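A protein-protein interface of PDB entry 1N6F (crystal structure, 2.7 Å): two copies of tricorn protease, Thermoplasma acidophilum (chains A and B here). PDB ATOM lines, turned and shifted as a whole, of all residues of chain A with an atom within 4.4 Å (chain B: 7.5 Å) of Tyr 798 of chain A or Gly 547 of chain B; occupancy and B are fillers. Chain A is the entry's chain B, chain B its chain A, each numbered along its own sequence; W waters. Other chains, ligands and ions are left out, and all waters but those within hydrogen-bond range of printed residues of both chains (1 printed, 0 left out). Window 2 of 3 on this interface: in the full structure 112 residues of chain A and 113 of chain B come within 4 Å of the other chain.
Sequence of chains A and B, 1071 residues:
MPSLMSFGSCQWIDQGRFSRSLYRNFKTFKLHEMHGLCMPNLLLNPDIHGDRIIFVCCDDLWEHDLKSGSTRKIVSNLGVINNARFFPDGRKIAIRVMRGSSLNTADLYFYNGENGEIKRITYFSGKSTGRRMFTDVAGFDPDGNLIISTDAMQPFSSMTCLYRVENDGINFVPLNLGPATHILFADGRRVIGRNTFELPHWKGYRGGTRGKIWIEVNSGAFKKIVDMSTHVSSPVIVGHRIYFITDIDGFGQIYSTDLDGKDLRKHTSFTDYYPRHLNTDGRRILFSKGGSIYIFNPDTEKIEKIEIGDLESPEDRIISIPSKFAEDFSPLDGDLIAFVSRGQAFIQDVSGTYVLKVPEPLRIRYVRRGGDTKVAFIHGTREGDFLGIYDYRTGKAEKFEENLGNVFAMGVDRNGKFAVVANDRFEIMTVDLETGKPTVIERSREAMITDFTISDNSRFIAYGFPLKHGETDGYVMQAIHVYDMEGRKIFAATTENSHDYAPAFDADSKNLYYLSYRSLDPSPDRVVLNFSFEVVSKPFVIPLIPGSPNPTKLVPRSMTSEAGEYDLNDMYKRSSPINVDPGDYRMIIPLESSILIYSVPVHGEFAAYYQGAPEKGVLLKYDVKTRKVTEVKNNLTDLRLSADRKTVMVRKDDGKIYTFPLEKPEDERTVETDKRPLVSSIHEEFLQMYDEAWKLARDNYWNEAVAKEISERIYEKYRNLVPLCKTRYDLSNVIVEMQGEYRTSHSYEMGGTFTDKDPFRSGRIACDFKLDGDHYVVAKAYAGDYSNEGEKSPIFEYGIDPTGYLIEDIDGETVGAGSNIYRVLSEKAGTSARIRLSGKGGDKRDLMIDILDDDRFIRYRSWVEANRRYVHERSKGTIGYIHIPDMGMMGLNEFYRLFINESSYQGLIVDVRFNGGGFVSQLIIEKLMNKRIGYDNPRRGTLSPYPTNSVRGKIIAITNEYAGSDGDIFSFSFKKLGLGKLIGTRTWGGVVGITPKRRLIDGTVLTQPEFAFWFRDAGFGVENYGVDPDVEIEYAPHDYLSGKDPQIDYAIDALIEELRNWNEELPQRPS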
ATOM      1  N   ILE A 795       4.888 -25.224 -16.450  1.00  0.00           N
ATOM      2  CA  ILE A 795       3.590 -25.857 -16.247  1.00  0.00           C
ATOM      3  C   ILE A 795       3.738 -27.376 -16.078  1.00  0.00           C
ATOM      4  O   ILE A 795       3.039 -27.974 -15.254  1.00  0.00           O
ATOM      5  CB  ILE A 795       2.608 -25.574 -17.426  1.00  0.00           C
ATOM      6  CG1 ILE A 795       2.094 -24.142 -17.346  1.00  0.00           C
ATOM      7  CG2 ILE A 795       1.424 -26.511 -17.376  1.00  0.00           C
ATOM      8  CD1 ILE A 795       1.191 -23.752 -18.487  1.00  0.00           C
ATOM      9  N   PHE A 796       4.642 -27.995 -16.838  1.00  0.00           N
ATOM     10  CA  PHE A 796       4.824 -29.451 -16.758  1.00  0.00           C
ATOM     11  C   PHE A 796       4.946 -30.010 -15.332  1.00  0.00           C
ATOM     12  O   PHE A 796       4.532 -31.132 -15.070  1.00  0.00           O
ATOM     13  CB  PHE A 796       6.041 -29.914 -17.574  1.00  0.00           C
ATOM     14  CG  PHE A 796       5.814 -29.962 -19.061  1.00  0.00           C
ATOM     15  CD1 PHE A 796       6.360 -28.998 -19.897  1.00  0.00           C
ATOM     16  CD2 PHE A 796       5.125 -31.020 -19.636  1.00  0.00           C
ATOM     17  CE1 PHE A 796       6.226 -29.104 -21.294  1.00  0.00           C
ATOM     18  CE2 PHE A 796       4.983 -31.138 -21.031  1.00  0.00           C
ATOM     19  CZ  PHE A 796       5.531 -30.186 -21.852  1.00  0.00           C
ATOM     20  N   GLU A 797       5.500 -29.233 -14.407  1.00  0.00           N
ATOM     21  CA  GLU A 797       5.657 -29.703 -13.033  1.00  0.00           C
ATOM     22  C   GLU A 797       4.357 -30.095 -12.355  1.00  0.00           C
ATOM     23  O   GLU A 797       4.372 -30.743 -11.297  1.00  0.00           O
ATOM     24  CB  GLU A 797       6.389 -28.666 -12.178  1.00  0.00           C
ATOM     25  CG  GLU A 797       7.872 -28.580 -12.545  1.00  0.00           C
ATOM     26  CD  GLU A 797       8.733 -27.908 -11.487  1.00  0.00           C
ATOM     27  OE1 GLU A 797       9.929 -27.707 -11.756  1.00  0.00           O
ATOM     28  OE2 GLU A 797       8.221 -27.589 -10.398  1.00  0.00           O
ATOM     29  N   TYR A 798       3.228 -29.712 -12.951  1.00  0.00           N
ATOM     30  CA  TYR A 798       1.917 -30.062 -12.390  1.00  0.00           C
ATOM     31  C   TYR A 798       1.341 -31.289 -13.061  1.00  0.00           C
ATOM     32  O   TYR A 798       0.159 -31.576 -12.937  1.00  0.00           O
ATOM     33  CB  TYR A 798       0.933 -28.900 -12.521  1.00  0.00           C
ATOM     34  CG  TYR A 798       1.168 -27.802 -11.518  1.00  0.00           C
ATOM     35  CD1 TYR A 798       2.017 -26.743 -11.803  1.00  0.00           C
ATOM     36  CD2 TYR A 798       0.582 -27.854 -10.265  1.00  0.00           C
ATOM     37  CE1 TYR A 798       2.278 -25.761 -10.865  1.00  0.00           C
ATOM     38  CE2 TYR A 798       0.839 -26.882  -9.317  1.00  0.00           C
ATOM     39  CZ  TYR A 798       1.690 -25.835  -9.626  1.00  0.00           C
ATOM     40  OH  TYR A 798       1.944 -24.873  -8.684  1.00  0.00           O
ATOM     41  N   GLY A 799       2.185 -32.009 -13.780  1.00  0.00           N
ATOM     42  CA  GLY A 799       1.731 -33.212 -14.433  1.00  0.00           C
ATOM     43  C   GLY A 799       0.742 -33.069 -15.562  1.00  0.00           C
ATOM     44  O   GLY A 799      -0.244 -33.793 -15.587  1.00  0.00           O
ATOM     45  N   ILE A 800       0.997 -32.154 -16.492  1.00  0.00           N
ATOM     46  CA  ILE A 800       0.110 -31.960 -17.646  1.00  0.00           C
ATOM     47  C   ILE A 800       0.833 -31.191 -18.731  1.00  0.00           C
ATOM     48  O   ILE A 800       1.616 -30.285 -18.442  1.00  0.00           O
ATOM     49  CB  ILE A 800      -1.158 -31.137 -17.321  1.00  0.00           C
ATOM     50  CG1 ILE A 800      -0.760 -29.897 -16.535  1.00  0.00           C
ATOM     51  CG2 ILE A 800      -2.184 -31.987 -16.600  1.00  0.00           C
ATOM     52  CD1 ILE A 800      -1.649 -28.709 -16.834  1.00  0.00           C
ATOM     53  N   LEU A 847      -3.529 -23.458 -11.639  1.00  0.00           N
ATOM     54  CA  LEU A 847      -2.182 -23.629 -11.113  1.00  0.00           C
ATOM     55  C   LEU A 847      -1.394 -22.348 -10.807  1.00  0.00           C
ATOM     56  O   LEU A 847      -1.649 -21.290 -11.381  1.00  0.00           O
ATOM     57  CB  LEU A 847      -1.381 -24.454 -12.111  1.00  0.00           C
ATOM     58  CG  LEU A 847      -2.230 -25.312 -13.042  1.00  0.00           C
ATOM     59  CD1 LEU A 847      -1.414 -25.748 -14.236  1.00  0.00           C
ATOM     60  CD2 LEU A 847      -2.757 -26.510 -12.288  1.00  0.00           C
ATOM     61  N   MET A 848      -0.428 -22.461  -9.894  1.00  0.00           N
ATOM     62  CA  MET A 848       0.445 -21.345  -9.536  1.00  0.00           C
ATOM     63  C   MET A 848       1.732 -21.563 -10.322  1.00  0.00           C
ATOM     64  O   MET A 848       2.679 -22.213  -9.854  1.00  0.00           O
ATOM     65  CB  MET A 848       0.759 -21.329  -8.040  1.00  0.00           C
ATOM     66  CG  MET A 848      -0.360 -20.810  -7.133  1.00  0.00           C
ATOM     67  SD  MET A 848      -0.821 -19.061  -7.386  1.00  0.00           S
ATOM     68  CE  MET A 848       0.549 -18.224  -6.598  1.00  0.00           C
ATOM     69  N   ILE A 849       1.745 -21.021 -11.534  1.00  0.00           N
ATOM     70  CA  ILE A 849       2.876 -21.156 -12.431  1.00  0.00           C
ATOM     71  C   ILE A 849       3.960 -20.133 -12.180  1.00  0.00           C
ATOM     72  O   ILE A 849       3.690 -18.988 -11.865  1.00  0.00           O
ATOM     73  CB  ILE A 849       2.431 -21.001 -13.873  1.00  0.00           C
ATOM     74  CG1 ILE A 849       1.271 -21.947 -14.143  1.00  0.00           C
ATOM     75  CG2 ILE A 849       3.597 -21.283 -14.807  1.00  0.00           C
ATOM     76  CD1 ILE A 849       1.589 -23.393 -13.836  1.00  0.00           C
ATOM     77  N   PRO B 543       6.811 -35.455  -6.971  1.00  0.00           N
ATOM     78  CA  PRO B 543       5.610 -35.708  -6.156  1.00  0.00           C
ATOM     79  C   PRO B 543       4.835 -36.883  -6.746  1.00  0.00           C
ATOM     80  O   PRO B 543       4.573 -36.939  -7.942  1.00  0.00           O
ATOM     81  CB  PRO B 543       4.841 -34.380  -6.208  1.00  0.00           C
ATOM     82  CG  PRO B 543       5.351 -33.734  -7.474  1.00  0.00           C
ATOM     83  CD  PRO B 543       6.809 -34.094  -7.521  1.00  0.00           C
ATOM     84  N   LEU B 544       4.520 -37.845  -5.893  1.00  0.00           N
ATOM     85  CA  LEU B 544       3.825 -39.038  -6.316  1.00  0.00           C
ATOM     86  C   LEU B 544       2.371 -38.763  -6.669  1.00  0.00           C
ATOM     87  O   LEU B 544       1.715 -39.592  -7.305  1.00  0.00           O
ATOM     88  CB  LEU B 544       3.954 -40.100  -5.232  1.00  0.00           C
ATOM     89  CG  LEU B 544       5.421 -40.382  -4.875  1.00  0.00           C
ATOM     90  CD1 LEU B 544       5.507 -41.656  -4.026  1.00  0.00           C
ATOM     91  CD2 LEU B 544       6.254 -40.548  -6.159  1.00  0.00           C
ATOM     92  N   ILE B 545       1.868 -37.594  -6.275  1.00  0.00           N
ATOM     93  CA  ILE B 545       0.502 -37.230  -6.616  1.00  0.00           C
ATOM     94  C   ILE B 545       0.505 -36.042  -7.581  1.00  0.00           C
ATOM     95  O   ILE B 545       0.837 -34.912  -7.204  1.00  0.00           O
ATOM     96  CB  ILE B 545      -0.339 -36.832  -5.381  1.00  0.00           C
ATOM     97  CG1 ILE B 545      -0.476 -37.998  -4.419  1.00  0.00           C
ATOM     98  CG2 ILE B 545      -1.718 -36.397  -5.833  1.00  0.00           C
ATOM     99  CD1 ILE B 545       0.726 -38.243  -3.580  1.00  0.00           C
ATOM    100  N   PRO B 546       0.140 -36.287  -8.844  1.00  0.00           N
ATOM    101  CA  PRO B 546       0.105 -35.228  -9.850  1.00  0.00           C
ATOM    102  C   PRO B 546      -0.634 -34.007  -9.334  1.00  0.00           C
ATOM    103  O   PRO B 546      -1.676 -34.141  -8.680  1.00  0.00           O
ATOM    104  CB  PRO B 546      -0.646 -35.875 -10.999  1.00  0.00           C
ATOM    105  CG  PRO B 546      -0.256 -37.270 -10.911  1.00  0.00           C
ATOM    106  CD  PRO B 546      -0.277 -37.570  -9.422  1.00  0.00           C
ATOM    107  N   GLY B 547      -0.108 -32.820  -9.633  1.00  0.00           N
ATOM    108  CA  GLY B 547      -0.769 -31.583  -9.220  1.00  0.00           C
ATOM    109  C   GLY B 547      -0.232 -31.057  -7.922  1.00  0.00           C
ATOM    110  O   GLY B 547      -0.440 -29.905  -7.563  1.00  0.00           O
ATOM    111  N   SER B 548       0.465 -31.930  -7.213  1.00  0.00           N
ATOM    112  CA  SER B 548       1.048 -31.561  -5.948  1.00  0.00           C
ATOM    113  C   SER B 548       2.383 -30.939  -6.321  1.00  0.00           C
ATOM    114  O   SER B 548       3.128 -31.480  -7.127  1.00  0.00           O
ATOM    115  CB  SER B 548       1.214 -32.801  -5.079  1.00  0.00           C
ATOM    116  OG  SER B 548       1.374 -32.429  -3.744  1.00  0.00           O
ATOM    117  N   PRO B 549       2.687 -29.770  -5.761  1.00  0.00           N
ATOM    118  CA  PRO B 549       3.947 -29.113  -6.084  1.00  0.00           C
ATOM    119  C   PRO B 549       5.131 -29.602  -5.255  1.00  0.00           C
ATOM    120  O   PRO B 549       4.975 -30.346  -4.284  1.00  0.00           O
ATOM    121  CB  PRO B 549       3.630 -27.642  -5.822  1.00  0.00           C
ATOM    122  CG  PRO B 549       2.762 -27.729  -4.607  1.00  0.00           C
ATOM    123  CD  PRO B 549       1.842 -28.904  -4.922  1.00  0.00           C
ATOM    124  N   ASN B 550       6.317 -29.168  -5.665  1.00  0.00           N
ATOM    125  CA  ASN B 550       7.558 -29.485  -4.984  1.00  0.00           C
ATOM    126  C   ASN B 550       7.509 -28.821  -3.600  1.00  0.00           C
ATOM    127  O   ASN B 550       7.546 -27.592  -3.464  1.00  0.00           O
ATOM    128  CB  ASN B 550       8.725 -28.925  -5.805  1.00  0.00           C
ATOM    129  CG  ASN B 550      10.023 -28.870  -5.030  1.00  0.00           C
ATOM    130  OD1 ASN B 550      10.035 -28.944  -3.799  1.00  0.00           O
ATOM    131  ND2 ASN B 550      11.129 -28.709  -5.746  1.00  0.00           N
ATOM    132  N   LYS B 553       9.531 -25.821  -2.457  1.00  0.00           N
ATOM    133  CA  LYS B 553       9.172 -24.551  -3.069  1.00  0.00           C
ATOM    134  C   LYS B 553       8.368 -23.626  -2.156  1.00  0.00           C
ATOM    135  O   LYS B 553       8.220 -22.425  -2.441  1.00  0.00           O
ATOM    136  CB  LYS B 553       8.384 -24.775  -4.357  1.00  0.00           C
ATOM    137  CG  LYS B 553       9.257 -25.061  -5.561  1.00  0.00           C
ATOM    138  CD  LYS B 553       8.485 -24.815  -6.836  1.00  0.00           C
ATOM    139  CE  LYS B 553       9.399 -24.705  -8.022  1.00  0.00           C
ATOM    140  NZ  LYS B 553       8.653 -24.167  -9.192  1.00  0.00           N
ATOM    141  N   VAL B 555       5.119 -23.462  -1.608  1.00  0.00           N
ATOM    142  CA  VAL B 555       3.912 -22.936  -2.240  1.00  0.00           C
ATOM    143  C   VAL B 555       2.760 -22.991  -1.238  1.00  0.00           C
ATOM    144  O   VAL B 555       2.330 -24.074  -0.852  1.00  0.00           O
ATOM    145  CB  VAL B 555       3.514 -23.769  -3.458  1.00  0.00           C
ATOM    146  CG1 VAL B 555       2.436 -23.070  -4.236  1.00  0.00           C
ATOM    147  CG2 VAL B 555       4.717 -24.008  -4.329  1.00  0.00           C
ATOM    148  N   ARG B 557      -0.208 -23.566   0.980  1.00  0.00           N
ATOM    149  CA  ARG B 557      -1.193 -24.635   0.884  1.00  0.00           C
ATOM    150  C   ARG B 557      -2.537 -24.121   0.405  1.00  0.00           C
ATOM    151  O   ARG B 557      -3.189 -24.748  -0.416  1.00  0.00           O
ATOM    152  CB  ARG B 557      -1.354 -25.346   2.238  1.00  0.00           C
ATOM    153  CG  ARG B 557      -2.548 -26.330   2.299  1.00  0.00           C
ATOM    154  CD  ARG B 557      -2.540 -27.368   1.150  1.00  0.00           C
ATOM    155  NE  ARG B 557      -3.825 -28.071   1.000  1.00  0.00           N
ATOM    156  CZ  ARG B 557      -4.227 -28.683  -0.117  1.00  0.00           C
ATOM    157  NH1 ARG B 557      -5.411 -29.288  -0.154  1.00  0.00           N
ATOM    158  NH2 ARG B 557      -3.455 -28.680  -1.206  1.00  0.00           N
ATOM    159  N   MET B 559      -3.124 -21.946  -1.568  1.00  0.00           N
ATOM    160  CA  MET B 559      -3.046 -21.588  -2.970  1.00  0.00           C
ATOM    161  C   MET B 559      -2.836 -22.792  -3.880  1.00  0.00           C
ATOM    162  O   MET B 559      -2.545 -22.639  -5.067  1.00  0.00           O
ATOM    163  CB  MET B 559      -1.929 -20.560  -3.190  1.00  0.00           C
ATOM    164  CG  MET B 559      -2.256 -19.165  -2.686  1.00  0.00           C
ATOM    165  SD  MET B 559      -0.915 -18.030  -3.044  1.00  0.00           S
ATOM    166  CE  MET B 559      -0.846 -17.101  -1.486  1.00  0.00           C
ATOM    167  N   THR B 560      -2.977 -23.988  -3.326  1.00  0.00           N
ATOM    168  CA  THR B 560      -2.823 -25.217  -4.101  1.00  0.00           C
ATOM    169  C   THR B 560      -4.013 -26.138  -3.838  1.00  0.00           C
ATOM    170  O   THR B 560      -4.726 -25.984  -2.842  1.00  0.00           O
ATOM    171  CB  THR B 560      -1.516 -25.971  -3.747  1.00  0.00           C
ATOM    172  OG1 THR B 560      -1.512 -26.315  -2.360  1.00  0.00           O
ATOM    173  CG2 THR B 560      -0.321 -25.103  -4.044  1.00  0.00           C
ATOM    174  N   SER B 561      -4.231 -27.091  -4.738  1.00  0.00           N
ATOM    175  CA  SER B 561      -5.338 -28.032  -4.599  1.00  0.00           C
ATOM    176  C   SER B 561      -4.849 -29.466  -4.761  1.00  0.00           C
ATOM    177  O   SER B 561      -5.039 -30.081  -5.819  1.00  0.00           O
ATOM    178  CB  SER B 561      -6.408 -27.733  -5.648  1.00  0.00           C
ATOM    179  OG  SER B 561      -5.837 -27.725  -6.945  1.00  0.00           O
ATOM    180  N   GLU B 562      -4.218 -30.003  -3.722  1.00  0.00           N
ATOM    181  CA  GLU B 562      -3.713 -31.376  -3.792  1.00  0.00           C
ATOM    182  C   GLU B 562      -4.838 -32.390  -3.590  1.00  0.00           C
ATOM    183  O   GLU B 562      -5.797 -32.442  -4.368  1.00  0.00           O
ATOM    184  CB  GLU B 562      -2.610 -31.602  -2.740  1.00  0.00           C
ATOM    185  N   ALA B 563      -4.698 -33.194  -2.540  1.00  0.00           N
ATOM    186  CA  ALA B 563      -5.683 -34.210  -2.203  1.00  0.00           C
ATOM    187  C   ALA B 563      -5.894 -35.209  -3.343  1.00  0.00           C
ATOM    188  O   ALA B 563      -6.726 -36.115  -3.227  1.00  0.00           O
ATOM    189  CB  ALA B 563      -7.015 -33.548  -1.824  1.00  0.00           C
ATOM    190  N   GLY B 564      -5.154 -35.042  -4.440  1.00  0.00           N
ATOM    191  CA  GLY B 564      -5.280 -35.964  -5.555  1.00  0.00           C
ATOM    192  C   GLY B 564      -4.971 -37.382  -5.102  1.00  0.00           C
ATOM    193  O   GLY B 564      -4.826 -37.653  -3.904  1.00  0.00           O
ATOM    194  N   LYS B 573       8.187 -36.050 -15.794  1.00  0.00           N
ATOM    195  CA  LYS B 573       7.863 -34.737 -16.346  1.00  0.00           C
ATOM    196  C   LYS B 573       7.578 -33.746 -15.232  1.00  0.00           C
ATOM    197  O   LYS B 573       7.739 -32.552 -15.437  1.00  0.00           O
ATOM    198  CB  LYS B 573       6.640 -34.818 -17.260  1.00  0.00           C
ATOM    199  CG  LYS B 573       6.814 -35.719 -18.456  1.00  0.00           C
ATOM    200  CD  LYS B 573       5.633 -35.582 -19.400  1.00  0.00           C
ATOM    201  CE  LYS B 573       5.837 -36.423 -20.650  1.00  0.00           C
ATOM    202  NZ  LYS B 573       4.662 -36.397 -21.565  1.00  0.00           N
ATOM    203  N   ARG B 574       7.168 -34.247 -14.062  1.00  0.00           N
ATOM    204  CA  ARG B 574       6.838 -33.398 -12.919  1.00  0.00           C
ATOM    205  C   ARG B 574       8.060 -33.139 -12.056  1.00  0.00           C
ATOM    206  O   ARG B 574       7.975 -32.438 -11.034  1.00  0.00           O
ATOM    207  CB  ARG B 574       5.794 -34.051 -12.025  1.00  0.00           C
ATOM    208  CG  ARG B 574       4.685 -34.751 -12.733  1.00  0.00           C
ATOM    209  CD  ARG B 574       3.531 -34.990 -11.743  1.00  0.00           C
ATOM    210  NE  ARG B 574       3.696 -36.123 -10.827  1.00  0.00           N
ATOM    211  CZ  ARG B 574       3.410 -37.386 -11.131  1.00  0.00           C
ATOM    212  NH1 ARG B 574       3.588 -38.341 -10.233  1.00  0.00           N
ATOM    213  NH2 ARG B 574       2.941 -37.701 -12.326  1.00  0.00           N
ATOM    214  N   SER B 575       9.187 -33.724 -12.452  1.00  0.00           N
ATOM    215  CA  SER B 575      10.420 -33.558 -11.698  1.00  0.00           C
ATOM    216  C   SER B 575      10.676 -32.088 -11.442  1.00  0.00           C
ATOM    217  O   SER B 575      10.298 -31.218 -12.240  1.00  0.00           O
ATOM    218  CB  SER B 575      11.602 -34.128 -12.470  1.00  0.00           C
ATOM    219  OG  SER B 575      11.750 -33.377 -13.667  1.00  0.00           O
HETATM  220  O   HOH W   1       2.783 -32.212  -9.692  1.00  0.00           O
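The side-chain carboxylate (OE2) of Glu 797 of chain A is in salt-bridge range of the side-chain amino group (NZ) of Lys 553 of chain B, at 3.7 Å.
The guanidinium group (NH1) of Arg 574 of chain B lies within hydrogen-bond range of the backbone carbonyl oxygen (O) of Pro 543 of chain B.
The backbone NH (N) of Lys 553 of chain B sits at hydrogen-bond distance from the side-chain amide oxygen (OD1) of Asn 550 of chain B (3.4 Å).
The side-chain hydroxyl (OH) of Tyr 798 of chain A sits at hydrogen-bond distance from the backbone carbonyl oxygen (O) of Met 848 of chain A (3.0 Å).
O of Phe 796 of chain A touches O of Lys 573 of chain B, at 3.5 Å.
Arg 574 of chain B touches Phe 796 of chain A (CA to O, 3.9 Å).
Glu 797 of chain A touches Arg 574 of chain B (O to CB, 3.7 Å).
Ser 575 of chain B touches Glu 797 of chain A (O to OE1, 3.6 Å).
Tyr 798 of chain A touches Gly 547 of chain B (O to N, 3.5 Å).
Gly 799 of chain A touches Arg 574 of chain B.
Met 848 of chain A touches Met 559 of chain B.
Of chain B, only Gly 547 comes within 4 Å of Tyr 798 of chain A.
Printed residues of chain B within 4 Å of Gly 799 of chain A: Arg 574 (3.7 Å).
Printed residues of chain A within 4 Å of Lys 553 of chain B: Glu 797 (3.7 Å).
The nearest residue of chain B that does not touch Tyr 798 of chain A is Pro 549 of chain B (4.3 Å).
The nearest printed residue of chain A that does not touch Gly 547 of chain B is Gly 799 of chain A (4.8 Å).
The nearest printed residue of chain A that does not touch Met 559 of chain B is Leu 847 of chain A (5.9 Å).
Printed residues of chain A that touch a printed residue of chain B: Phe 796, Glu 797, Tyr 798, Gly 799 and Met 848.
Hydrophobic or aromatic side chains of chain B within 4 Å of the printed part of chain A: Met 559.
Among the printed residues, 8 pairs touch across the chains.
Among the printed residues, Asp or Glu carboxylates within 4 Å of a Lys or Arg side-chain nitrogen of the other chain: Glu 797 of chain A with Lys 553 of chain B (3.7 Å).
No position is printed for both chains.
Of the 8 pairs that touch across the chains among the printed residues, none has its exchanged pair printed and touching as well.
Water W1 lies within hydrogen-bond range of O of Ser 548 of chain B (2.7 Å), O of Glu 797 of chain A (2.7 Å) and N of Gly 547 of chain B (3.0 Å).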
